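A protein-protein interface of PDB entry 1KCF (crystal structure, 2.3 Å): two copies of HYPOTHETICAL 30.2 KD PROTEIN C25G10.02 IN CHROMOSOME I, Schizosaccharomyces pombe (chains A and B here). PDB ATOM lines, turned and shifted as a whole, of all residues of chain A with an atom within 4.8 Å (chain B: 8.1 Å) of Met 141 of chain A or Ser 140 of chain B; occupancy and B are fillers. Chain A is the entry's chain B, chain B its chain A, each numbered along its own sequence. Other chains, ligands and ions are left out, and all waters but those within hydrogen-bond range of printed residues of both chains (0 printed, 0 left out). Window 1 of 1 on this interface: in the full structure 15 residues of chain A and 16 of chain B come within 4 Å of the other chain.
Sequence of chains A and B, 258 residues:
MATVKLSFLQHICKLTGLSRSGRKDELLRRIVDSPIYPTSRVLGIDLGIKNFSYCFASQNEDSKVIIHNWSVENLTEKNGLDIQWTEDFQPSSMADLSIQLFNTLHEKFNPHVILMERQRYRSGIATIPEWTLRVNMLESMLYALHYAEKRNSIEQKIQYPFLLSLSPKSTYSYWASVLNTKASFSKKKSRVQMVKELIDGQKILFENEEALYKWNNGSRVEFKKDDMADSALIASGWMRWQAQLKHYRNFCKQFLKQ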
ATOM      1  N   PRO A  91     -19.525  -3.332   6.277  1.00  0.00           N
ATOM      2  CA  PRO A  91     -19.617  -2.243   7.258  1.00  0.00           C
ATOM      3  C   PRO A  91     -19.456  -2.663   8.722  1.00  0.00           C
ATOM      4  O   PRO A  91     -18.622  -2.107   9.445  1.00  0.00           O
ATOM      5  CB  PRO A  91     -20.993  -1.642   6.973  1.00  0.00           C
ATOM      6  CG  PRO A  91     -21.123  -1.820   5.491  1.00  0.00           C
ATOM      7  CD  PRO A  91     -20.610  -3.235   5.281  1.00  0.00           C
ATOM      8  N   MET A  94     -15.958  -3.711   9.363  1.00  0.00           N
ATOM      9  CA  MET A  94     -15.042  -2.573   9.334  1.00  0.00           C
ATOM     10  C   MET A  94     -15.160  -1.740  10.605  1.00  0.00           C
ATOM     11  O   MET A  94     -14.161  -1.241  11.128  1.00  0.00           O
ATOM     12  CB  MET A  94     -15.324  -1.694   8.113  1.00  0.00           C
ATOM     13  CG  MET A  94     -14.849  -2.282   6.790  1.00  0.00           C
ATOM     14  SD  MET A  94     -13.067  -2.556   6.748  1.00  0.00           S
ATOM     15  CE  MET A  94     -12.462  -0.895   6.375  1.00  0.00           C
ATOM     16  N   ALA A  95     -16.385  -1.586  11.096  1.00  0.00           N
ATOM     17  CA  ALA A  95     -16.609  -0.826  12.314  1.00  0.00           C
ATOM     18  C   ALA A  95     -15.836  -1.488  13.450  1.00  0.00           C
ATOM     19  O   ALA A  95     -15.256  -0.806  14.289  1.00  0.00           O
ATOM     20  CB  ALA A  95     -18.096  -0.779  12.641  1.00  0.00           C
ATOM     21  N   SER A  98     -12.287  -0.531  13.069  1.00  0.00           N
ATOM     22  CA  SER A  98     -12.136   0.880  13.412  1.00  0.00           C
ATOM     23  C   SER A  98     -12.082   1.106  14.916  1.00  0.00           C
ATOM     24  O   SER A  98     -11.229   1.840  15.413  1.00  0.00           O
ATOM     25  CB  SER A  98     -13.289   1.689  12.824  1.00  0.00           C
ATOM     26  OG  SER A  98     -13.208   1.711  11.413  1.00  0.00           O
ATOM     27  N   MET A 137     -13.396   3.970   4.081  1.00  0.00           N
ATOM     28  CA  MET A 137     -14.357   3.537   5.088  1.00  0.00           C
ATOM     29  C   MET A 137     -13.702   3.581   6.465  1.00  0.00           C
ATOM     30  O   MET A 137     -14.272   4.104   7.420  1.00  0.00           O
ATOM     31  CB  MET A 137     -14.856   2.114   4.789  1.00  0.00           C
ATOM     32  CG  MET A 137     -16.053   1.692   5.637  1.00  0.00           C
ATOM     33  SD  MET A 137     -16.801   0.102   5.150  1.00  0.00           S
ATOM     34  CE  MET A 137     -16.688   0.219   3.359  1.00  0.00           C
ATOM     35  N   LEU A 138     -12.495   3.035   6.560  1.00  0.00           N
ATOM     36  CA  LEU A 138     -11.764   3.021   7.819  1.00  0.00           C
ATOM     37  C   LEU A 138     -11.521   4.465   8.265  1.00  0.00           C
ATOM     38  O   LEU A 138     -11.664   4.796   9.438  1.00  0.00           O
ATOM     39  CB  LEU A 138     -10.427   2.291   7.642  1.00  0.00           C
ATOM     40  CG  LEU A 138      -9.492   2.200   8.857  1.00  0.00           C
ATOM     41  CD1 LEU A 138     -10.169   1.443   9.976  1.00  0.00           C
ATOM     42  CD2 LEU A 138      -8.196   1.499   8.458  1.00  0.00           C
ATOM     43  N   GLU A 139     -11.162   5.317   7.312  1.00  0.00           N
ATOM     44  CA  GLU A 139     -10.895   6.721   7.588  1.00  0.00           C
ATOM     45  C   GLU A 139     -12.139   7.425   8.120  1.00  0.00           C
ATOM     46  O   GLU A 139     -12.080   8.130   9.121  1.00  0.00           O
ATOM     47  CB  GLU A 139     -10.423   7.433   6.317  1.00  0.00           C
ATOM     48  CG  GLU A 139     -10.011   8.880   6.544  1.00  0.00           C
ATOM     49  CD  GLU A 139      -9.856   9.659   5.245  1.00  0.00           C
ATOM     50  OE1 GLU A 139      -9.194  10.716   5.260  1.00  0.00           O
ATOM     51  OE2 GLU A 139     -10.404   9.221   4.210  1.00  0.00           O
ATOM     52  N   SER A 140     -13.265   7.233   7.443  1.00  0.00           N
ATOM     53  CA  SER A 140     -14.511   7.864   7.856  1.00  0.00           C
ATOM     54  C   SER A 140     -14.945   7.439   9.259  1.00  0.00           C
ATOM     55  O   SER A 140     -15.441   8.253  10.029  1.00  0.00           O
ATOM     56  CB  SER A 140     -15.621   7.540   6.861  1.00  0.00           C
ATOM     57  OG  SER A 140     -15.305   8.020   5.573  1.00  0.00           O
ATOM     58  N   MET A 141     -14.759   6.163   9.580  1.00  0.00           N
ATOM     59  CA  MET A 141     -15.141   5.648  10.887  1.00  0.00           C
ATOM     60  C   MET A 141     -14.247   6.206  11.991  1.00  0.00           C
ATOM     61  O   MET A 141     -14.725   6.508  13.081  1.00  0.00           O
ATOM     62  CB  MET A 141     -15.093   4.118  10.888  1.00  0.00           C
ATOM     63  CG  MET A 141     -16.104   3.493   9.945  1.00  0.00           C
ATOM     64  SD  MET A 141     -16.149   1.709  10.066  1.00  0.00           S
ATOM     65  CE  MET A 141     -17.713   1.368   9.212  1.00  0.00           C
ATOM     66  N   LEU A 142     -12.954   6.343  11.706  1.00  0.00           N
ATOM     67  CA  LEU A 142     -12.023   6.894  12.683  1.00  0.00           C
ATOM     68  C   LEU A 142     -12.403   8.345  12.968  1.00  0.00           C
ATOM     69  O   LEU A 142     -12.337   8.793  14.112  1.00  0.00           O
ATOM     70  CB  LEU A 142     -10.581   6.823  12.164  1.00  0.00           C
ATOM     71  CG  LEU A 142      -9.956   5.424  12.088  1.00  0.00           C
ATOM     72  CD1 LEU A 142      -8.510   5.525  11.587  1.00  0.00           C
ATOM     73  CD2 LEU A 142     -10.005   4.764  13.471  1.00  0.00           C
ATOM     74  N   TYR A 143     -12.799   9.075  11.926  1.00  0.00           N
ATOM     75  CA  TYR A 143     -13.200  10.469  12.081  1.00  0.00           C
ATOM     76  C   TYR A 143     -14.447  10.582  12.946  1.00  0.00           C
ATOM     77  O   TYR A 143     -14.521  11.439  13.818  1.00  0.00           O
ATOM     78  CB  TYR A 143     -13.480  11.114  10.720  1.00  0.00           C
ATOM     79  CG  TYR A 143     -12.269  11.729  10.072  1.00  0.00           C
ATOM     80  CD1 TYR A 143     -11.621  12.817  10.657  1.00  0.00           C
ATOM     81  CD2 TYR A 143     -11.750  11.213   8.887  1.00  0.00           C
ATOM     82  CE1 TYR A 143     -10.480  13.370  10.081  1.00  0.00           C
ATOM     83  CE2 TYR A 143     -10.607  11.761   8.304  1.00  0.00           C
ATOM     84  CZ  TYR A 143      -9.978  12.836   8.907  1.00  0.00           C
ATOM     85  OH  TYR A 143      -8.833  13.361   8.348  1.00  0.00           O
ATOM     86  N   ALA A 144     -15.424   9.714  12.697  1.00  0.00           N
ATOM     87  CA  ALA A 144     -16.675   9.726  13.450  1.00  0.00           C
ATOM     88  C   ALA A 144     -16.444   9.423  14.928  1.00  0.00           C
ATOM     89  O   ALA A 144     -17.008  10.085  15.803  1.00  0.00           O
ATOM     90  CB  ALA A 144     -17.657   8.715  12.854  1.00  0.00           C
ATOM     91  N   LEU A 145     -15.619   8.414  15.197  1.00  0.00           N
ATOM     92  CA  LEU A 145     -15.310   8.029  16.565  1.00  0.00           C
ATOM     93  C   LEU A 145     -14.607   9.192  17.245  1.00  0.00           C
ATOM     94  O   LEU A 145     -14.948   9.564  18.363  1.00  0.00           O
ATOM     95  CB  LEU A 145     -14.407   6.797  16.572  1.00  0.00           C
ATOM     96  CG  LEU A 145     -15.061   5.491  16.107  1.00  0.00           C
ATOM     97  CD1 LEU A 145     -14.012   4.403  15.963  1.00  0.00           C
ATOM     98  CD2 LEU A 145     -16.125   5.081  17.115  1.00  0.00           C
ATOM     99  N   LEU B  47     -30.056   5.805   2.392  1.00  0.00           N
ATOM    100  CA  LEU B  47     -28.967   6.769   2.497  1.00  0.00           C
ATOM    101  C   LEU B  47     -28.831   7.739   1.332  1.00  0.00           C
ATOM    102  O   LEU B  47     -28.716   7.341   0.169  1.00  0.00           O
ATOM    103  CB  LEU B  47     -27.635   6.052   2.705  1.00  0.00           C
ATOM    104  CG  LEU B  47     -27.461   5.328   4.039  1.00  0.00           C
ATOM    105  CD1 LEU B  47     -26.157   4.548   4.019  1.00  0.00           C
ATOM    106  CD2 LEU B  47     -27.481   6.335   5.176  1.00  0.00           C
ATOM    107  N   ALA B  95     -18.918  14.089   9.873  1.00  0.00           N
ATOM    108  CA  ALA B  95     -19.030  13.488  11.196  1.00  0.00           C
ATOM    109  C   ALA B  95     -20.113  14.248  11.937  1.00  0.00           C
ATOM    110  O   ALA B  95     -20.935  13.661  12.635  1.00  0.00           O
ATOM    111  CB  ALA B  95     -17.709  13.597  11.936  1.00  0.00           C
ATOM    112  N   SER B  98     -23.404  13.139  10.558  1.00  0.00           N
ATOM    113  CA  SER B  98     -23.666  11.771  10.984  1.00  0.00           C
ATOM    114  C   SER B  98     -24.099  11.707  12.444  1.00  0.00           C
ATOM    115  O   SER B  98     -24.991  10.939  12.799  1.00  0.00           O
ATOM    116  CB  SER B  98     -22.422  10.906  10.787  1.00  0.00           C
ATOM    117  OG  SER B  98     -22.014  10.907   9.431  1.00  0.00           O
ATOM    118  N   MET B 116     -30.453  -0.359   6.636  1.00  0.00           N
ATOM    119  CA  MET B 116     -29.731   0.626   5.852  1.00  0.00           C
ATOM    120  C   MET B 116     -29.451   0.154   4.433  1.00  0.00           C
ATOM    121  O   MET B 116     -28.986  -0.960   4.201  1.00  0.00           O
ATOM    122  CB  MET B 116     -28.424   0.976   6.558  1.00  0.00           C
ATOM    123  CG  MET B 116     -27.889   2.365   6.256  1.00  0.00           C
ATOM    124  SD  MET B 116     -26.393   2.701   7.220  1.00  0.00           S
ATOM    125  CE  MET B 116     -27.116   3.171   8.788  1.00  0.00           C
ATOM    126  N   ARG B 118     -28.366   2.068   0.411  1.00  0.00           N
ATOM    127  CA  ARG B 118     -28.017   3.315  -0.260  1.00  0.00           C
ATOM    128  C   ARG B 118     -29.176   3.711  -1.158  1.00  0.00           C
ATOM    129  O   ARG B 118     -29.829   2.854  -1.752  1.00  0.00           O
ATOM    130  CB  ARG B 118     -26.765   3.149  -1.125  1.00  0.00           C
ATOM    131  CG  ARG B 118     -25.456   3.059  -0.368  1.00  0.00           C
ATOM    132  CD  ARG B 118     -24.299   2.849  -1.342  1.00  0.00           C
ATOM    133  NE  ARG B 118     -23.003   2.834  -0.671  1.00  0.00           N
ATOM    134  CZ  ARG B 118     -22.612   1.899   0.191  1.00  0.00           C
ATOM    135  NH1 ARG B 118     -23.418   0.887   0.493  1.00  0.00           N
ATOM    136  NH2 ARG B 118     -21.416   1.984   0.760  1.00  0.00           N
ATOM    137  N   LEU B 133     -18.671   9.029  -2.721  1.00  0.00           N
ATOM    138  CA  LEU B 133     -17.942   9.438  -1.525  1.00  0.00           C
ATOM    139  C   LEU B 133     -18.870   9.891  -0.400  1.00  0.00           C
ATOM    140  O   LEU B 133     -18.680   9.515   0.759  1.00  0.00           O
ATOM    141  CB  LEU B 133     -16.951  10.555  -1.871  1.00  0.00           C
ATOM    142  CG  LEU B 133     -15.702  10.114  -2.648  1.00  0.00           C
ATOM    143  CD1 LEU B 133     -14.942  11.330  -3.168  1.00  0.00           C
ATOM    144  CD2 LEU B 133     -14.810   9.266  -1.738  1.00  0.00           C
ATOM    145  N   ARG B 134     -19.872  10.693  -0.742  1.00  0.00           N
ATOM    146  CA  ARG B 134     -20.822  11.195   0.243  1.00  0.00           C
ATOM    147  C   ARG B 134     -21.589  10.077   0.943  1.00  0.00           C
ATOM    148  O   ARG B 134     -21.627  10.025   2.166  1.00  0.00           O
ATOM    149  CB  ARG B 134     -21.834  12.134  -0.412  1.00  0.00           C
ATOM    150  CG  ARG B 134     -21.241  13.334  -1.111  1.00  0.00           C
ATOM    151  CD  ARG B 134     -22.342  14.113  -1.820  1.00  0.00           C
ATOM    152  NE  ARG B 134     -21.813  15.172  -2.675  1.00  0.00           N
ATOM    153  CZ  ARG B 134     -22.567  16.026  -3.358  1.00  0.00           C
ATOM    154  NH1 ARG B 134     -23.890  15.948  -3.286  1.00  0.00           N
ATOM    155  NH2 ARG B 134     -22.001  16.958  -4.115  1.00  0.00           N
ATOM    156  N   VAL B 135     -22.205   9.188   0.167  1.00  0.00           N
ATOM    157  CA  VAL B 135     -22.984   8.101   0.748  1.00  0.00           C
ATOM    158  C   VAL B 135     -22.140   7.040   1.446  1.00  0.00           C
ATOM    159  O   VAL B 135     -22.586   6.443   2.426  1.00  0.00           O
ATOM    160  CB  VAL B 135     -23.878   7.406  -0.311  1.00  0.00           C
ATOM    161  CG1 VAL B 135     -24.886   8.399  -0.860  1.00  0.00           C
ATOM    162  CG2 VAL B 135     -23.020   6.834  -1.439  1.00  0.00           C
ATOM    163  N   ASN B 136     -20.934   6.792   0.945  1.00  0.00           N
ATOM    164  CA  ASN B 136     -20.074   5.799   1.578  1.00  0.00           C
ATOM    165  C   ASN B 136     -19.636   6.322   2.944  1.00  0.00           C
ATOM    166  O   ASN B 136     -19.552   5.571   3.917  1.00  0.00           O
ATOM    167  CB  ASN B 136     -18.834   5.519   0.720  1.00  0.00           C
ATOM    168  CG  ASN B 136     -19.171   4.817  -0.584  1.00  0.00           C
ATOM    169  OD1 ASN B 136     -20.277   4.303  -0.761  1.00  0.00           O
ATOM    170  ND2 ASN B 136     -18.209   4.781  -1.502  1.00  0.00           N
ATOM    171  N   MET B 137     -19.364   7.620   2.998  1.00  0.00           N
ATOM    172  CA  MET B 137     -18.923   8.268   4.218  1.00  0.00           C
ATOM    173  C   MET B 137     -20.028   8.275   5.268  1.00  0.00           C
ATOM    174  O   MET B 137     -19.786   7.969   6.433  1.00  0.00           O
ATOM    175  CB  MET B 137     -18.490   9.703   3.915  1.00  0.00           C
ATOM    176  CG  MET B 137     -17.488  10.255   4.899  1.00  0.00           C
ATOM    177  SD  MET B 137     -16.978  11.930   4.511  1.00  0.00           S
ATOM    178  CE  MET B 137     -16.218  11.672   2.900  1.00  0.00           C
ATOM    179  N   LEU B 138     -21.236   8.635   4.843  1.00  0.00           N
ATOM    180  CA  LEU B 138     -22.394   8.689   5.727  1.00  0.00           C
ATOM    181  C   LEU B 138     -22.643   7.312   6.330  1.00  0.00           C
ATOM    182  O   LEU B 138     -22.756   7.159   7.544  1.00  0.00           O
ATOM    183  CB  LEU B 138     -23.631   9.128   4.943  1.00  0.00           C
ATOM    184  CG  LEU B 138     -24.536  10.176   5.594  1.00  0.00           C
ATOM    185  CD1 LEU B 138     -25.863  10.216   4.846  1.00  0.00           C
ATOM    186  CD2 LEU B 138     -24.769   9.838   7.057  1.00  0.00           C
ATOM    187  N   GLU B 139     -22.725   6.312   5.465  1.00  0.00           N
ATOM    188  CA  GLU B 139     -22.948   4.941   5.895  1.00  0.00           C
ATOM    189  C   GLU B 139     -21.880   4.504   6.892  1.00  0.00           C
ATOM    190  O   GLU B 139     -22.193   3.987   7.964  1.00  0.00           O
ATOM    191  CB  GLU B 139     -22.932   4.009   4.680  1.00  0.00           C
ATOM    192  CG  GLU B 139     -22.904   2.529   5.016  1.00  0.00           C
ATOM    193  CD  GLU B 139     -22.913   1.649   3.777  1.00  0.00           C
ATOM    194  OE1 GLU B 139     -23.985   1.520   3.150  1.00  0.00           O
ATOM    195  OE2 GLU B 139     -21.851   1.094   3.422  1.00  0.00           O
ATOM    196  N   SER B 140     -20.619   4.718   6.526  1.00  0.00           N
ATOM    197  CA  SER B 140     -19.489   4.339   7.366  1.00  0.00           C
ATOM    198  C   SER B 140     -19.525   4.959   8.754  1.00  0.00           C
ATOM    199  O   SER B 140     -19.291   4.275   9.748  1.00  0.00           O
ATOM    200  CB  SER B 140     -18.172   4.719   6.691  1.00  0.00           C
ATOM    201  OG  SER B 140     -17.960   3.945   5.531  1.00  0.00           O
ATOM    202  N   MET B 141     -19.804   6.256   8.815  1.00  0.00           N
ATOM    203  CA  MET B 141     -19.851   6.956  10.090  1.00  0.00           C
ATOM    204  C   MET B 141     -21.011   6.486  10.967  1.00  0.00           C
ATOM    205  O   MET B 141     -20.838   6.285  12.171  1.00  0.00           O
ATOM    206  CB  MET B 141     -19.925   8.469   9.855  1.00  0.00           C
ATOM    207  CG  MET B 141     -18.698   9.014   9.122  1.00  0.00           C
ATOM    208  SD  MET B 141     -18.635  10.814   9.006  1.00  0.00           S
ATOM    209  CE  MET B 141     -16.892  11.077   8.671  1.00  0.00           C
ATOM    210  N   LEU B 142     -22.182   6.303  10.361  1.00  0.00           N
ATOM    211  CA  LEU B 142     -23.354   5.841  11.096  1.00  0.00           C
ATOM    212  C   LEU B 142     -23.080   4.477  11.720  1.00  0.00           C
ATOM    213  O   LEU B 142     -23.492   4.213  12.848  1.00  0.00           O
ATOM    214  CB  LEU B 142     -24.572   5.757  10.169  1.00  0.00           C
ATOM    215  CG  LEU B 142     -25.171   7.093   9.717  1.00  0.00           C
ATOM    216  CD1 LEU B 142     -26.358   6.829   8.810  1.00  0.00           C
ATOM    217  CD2 LEU B 142     -25.603   7.911  10.931  1.00  0.00           C
ATOM    218  N   TYR B 143     -22.378   3.620  10.986  1.00  0.00           N
ATOM    219  CA  TYR B 143     -22.034   2.288  11.467  1.00  0.00           C
ATOM    220  C   TYR B 143     -21.065   2.368  12.646  1.00  0.00           C
ATOM    221  O   TYR B 143     -21.216   1.655  13.647  1.00  0.00           O
ATOM    222  CB  TYR B 143     -21.404   1.472  10.340  1.00  0.00           C
ATOM    223  CG  TYR B 143     -22.305   0.389   9.804  1.00  0.00           C
ATOM    224  CD1 TYR B 143     -22.359  -0.863  10.416  1.00  0.00           C
ATOM    225  CD2 TYR B 143     -23.147   0.631   8.719  1.00  0.00           C
ATOM    226  CE1 TYR B 143     -23.231  -1.848   9.964  1.00  0.00           C
ATOM    227  CE2 TYR B 143     -24.023  -0.341   8.258  1.00  0.00           C
ATOM    228  CZ  TYR B 143     -24.062  -1.577   8.884  1.00  0.00           C
ATOM    229  OH  TYR B 143     -24.941  -2.536   8.440  1.00  0.00           O
ATOM    230  N   ALA B 144     -20.062   3.232  12.518  1.00  0.00           N
ATOM    231  CA  ALA B 144     -19.089   3.401  13.580  1.00  0.00           C
ATOM    232  C   ALA B 144     -19.801   3.889  14.839  1.00  0.00           C
ATOM    233  O   ALA B 144     -19.598   3.345  15.925  1.00  0.00           O
ATOM    234  CB  ALA B 144     -18.020   4.401  13.156  1.00  0.00           C
ATOM    235  N   LEU B 145     -20.641   4.910  14.695  1.00  0.00           N
ATOM    236  CA  LEU B 145     -21.362   5.446  15.841  1.00  0.00           C
ATOM    237  C   LEU B 145     -22.245   4.386  16.499  1.00  0.00           C
ATOM    238  O   LEU B 145     -22.323   4.303  17.723  1.00  0.00           O
ATOM    239  CB  LEU B 145     -22.216   6.649  15.425  1.00  0.00           C
ATOM    240  CG  LEU B 145     -21.441   7.906  15.012  1.00  0.00           C
ATOM    241  CD1 LEU B 145     -22.409   9.035  14.714  1.00  0.00           C
ATOM    242  CD2 LEU B 145     -20.489   8.310  16.125  1.00  0.00           C
ATOM    243  N   HIS B 146     -22.900   3.572  15.680  1.00  0.00           N
ATOM    244  CA  HIS B 146     -23.777   2.529  16.196  1.00  0.00           C
ATOM    245  C   HIS B 146     -23.013   1.487  17.010  1.00  0.00           C
ATOM    246  O   HIS B 146     -23.376   1.193  18.150  1.00  0.00           O
ATOM    247  CB  HIS B 146     -24.522   1.856  15.038  1.00  0.00           C
ATOM    248  CG  HIS B 146     -25.301   0.641  15.438  1.00  0.00           C
ATOM    249  ND1 HIS B 146     -24.747  -0.621  15.471  1.00  0.00           N
ATOM    250  CD2 HIS B 146     -26.588   0.499  15.834  1.00  0.00           C
ATOM    251  CE1 HIS B 146     -25.657  -1.489  15.870  1.00  0.00           C
ATOM    252  NE2 HIS B 146     -26.784  -0.835  16.098  1.00  0.00           N
ATOM    253  N   TYR B 147     -21.955   0.930  16.431  1.00  0.00           N
ATOM    254  CA  TYR B 147     -21.175  -0.077  17.130  1.00  0.00           C
ATOM    255  C   TYR B 147     -20.374   0.470  18.299  1.00  0.00           C
ATOM    256  O   TYR B 147     -20.053  -0.265  19.228  1.00  0.00           O
ATOM    257  CB  TYR B 147     -20.262  -0.822  16.155  1.00  0.00           C
ATOM    258  CG  TYR B 147     -20.997  -1.919  15.429  1.00  0.00           C
ATOM    259  CD1 TYR B 147     -21.624  -1.680  14.209  1.00  0.00           C
ATOM    260  CD2 TYR B 147     -21.128  -3.188  16.001  1.00  0.00           C
ATOM    261  CE1 TYR B 147     -22.368  -2.672  13.580  1.00  0.00           C
ATOM    262  CE2 TYR B 147     -21.874  -4.187  15.380  1.00  0.00           C
ATOM    263  CZ  TYR B 147     -22.489  -3.922  14.171  1.00  0.00           C
ATOM    264  OH  TYR B 147     -23.236  -4.902  13.556  1.00  0.00           O
ATOM    265  N   ALA B 148     -20.052   1.755  18.262  1.00  0.00           N
ATOM    266  CA  ALA B 148     -19.322   2.357  19.364  1.00  0.00           C
ATOM    267  C   ALA B 148     -20.298   2.458  20.531  1.00  0.00           C
ATOM    268  O   ALA B 148     -19.977   2.096  21.658  1.00  0.00           O
ATOM    269  CB  ALA B 148     -18.825   3.741  18.971  1.00  0.00           C
ATOM    270  N   LEU B 163     -28.668  -3.304  13.551  1.00  0.00           N
ATOM    271  CA  LEU B 163     -28.330  -2.480  12.401  1.00  0.00           C
ATOM    272  C   LEU B 163     -28.062  -3.471  11.288  1.00  0.00           C
ATOM    273  O   LEU B 163     -27.234  -4.362  11.439  1.00  0.00           O
ATOM    274  CB  LEU B 163     -27.074  -1.646  12.676  1.00  0.00           C
ATOM    275  CG  LEU B 163     -26.560  -0.770  11.529  1.00  0.00           C
ATOM    276  CD1 LEU B 163     -27.657   0.176  11.060  1.00  0.00           C
ATOM    277  CD2 LEU B 163     -25.341   0.020  11.992  1.00  0.00           C
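The backbone carbonyl oxygen (O) of Asn 136 of chain B sits at hydrogen-bond distance from the side-chain hydroxyl (OG) of Ser 140 of chain B.
The backbone NH of Ala 95 of chain A lies close to the side-chain sulfur of Met 141 of chain A (3.5 Å).
NH1 of Arg 118 of chain B lies within salt-bridge range of OE1 of Glu 139 of chain B (2.8 Å).
OG of Ser 98 of chain A lies close to SD of Met 141 of chain A (3.2 Å).
The side-chain hydroxyl (OG) of Ser 98 of chain B sits close to the side-chain sulfur (SD) of Met 141 of chain B (3.4 Å).
SD of Met 141 of chain B lies within hydrogen-bond range of N of Ala 95 of chain B, 3.4 Å away.
Among the printed residues, pairs that only touch across the chains: Pro 91 of chain A with Glu 139 of chain B, Pro 91 of chain A with Tyr 143 of chain B, Ala 95 of chain A with Tyr 147 of chain B, Met 137 of chain A with Ser 140 of chain B, Ser 140 of chain A with Met 137 of chain B, Ser 140 of chain A with Ser 140 of chain B, Ser 140 of chain A with Met 141 of chain B, Met 141 of chain A with Ser 140 of chain B, Met 141 of chain A with Tyr 143 of chain B, Met 141 of chain A with Ala 144 of chain B, Tyr 143 of chain A with Met 141 of chain B, Ala 144 of chain A with Met 141 of chain B, Ala 144 of chain A with Leu 145 of chain B and Leu 145 of chain A with Ala 148 of chain B.
Of chain B, only Ser 140, Tyr 143 and Ala 144 come within 4 Å of Met 141 of chain A.
Printed residues of chain A within 4 Å of Ser 140 of chain B: Met 137, Ser 140 and Met 141.
Printed residues of chain A within 4 Å of Tyr 143 of chain B: Pro 91 (3.5 Å) and Met 141 (3.9 Å).
Of the printed residues of chain B, Tyr 143 of chain A touches Met 141.
Of the printed residues of chain A, Met 141 of chain B touches Ser 140, Tyr 143 and Ala 144.
Printed residues of chain A within 4 Å of Tyr 147 of chain B: Ala 95.
Of the printed residues of chain B, Ala 144 of chain A touches Met 141 (3.8 Å) and Leu 145 (3.9 Å).
Arg 134 of chain B touches none of the printed residues of chain A.
Asn 136 of chain B touches none of the printed residues of chain A.
Of the 22 printed residues of chain B, 9 touch a printed residue of chain A.
Printed residues of chain B that touch a printed residue of chain A: Met 137, Glu 139, Ser 140, Met 141, Tyr 143, Ala 144, Leu 145, Tyr 147 and Ala 148.
Hydrophobic or aromatic side chains of chain B that line the printed part of chain A: Met 137, Met 141, Tyr 143, Ala 144, Leu 145, Tyr 147 and Ala 148.
Along chain B the printed residues that touch a printed residue of chain A span positions 137 to 148.
Along chain A the printed residues that touch a printed residue of chain B span positions 91 to 145.
Ser 140 of chain A touches its own counterpart, Ser 140 of chain B.
Met 141 of chain A touches Tyr 143 of chain B, and with the chains exchanged Tyr 143 of chain A touches Met 141 of chain B.
Met 141 of chain A touches Ala 144 of chain B, and with the chains exchanged Ala 144 of chain A touches Met 141 of chain B.
Ala 144 of chain A touches Leu 145 of chain B, but with the chains exchanged Leu 145 of chain A does not touch Ala 144 of chain B (4.1 Å).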
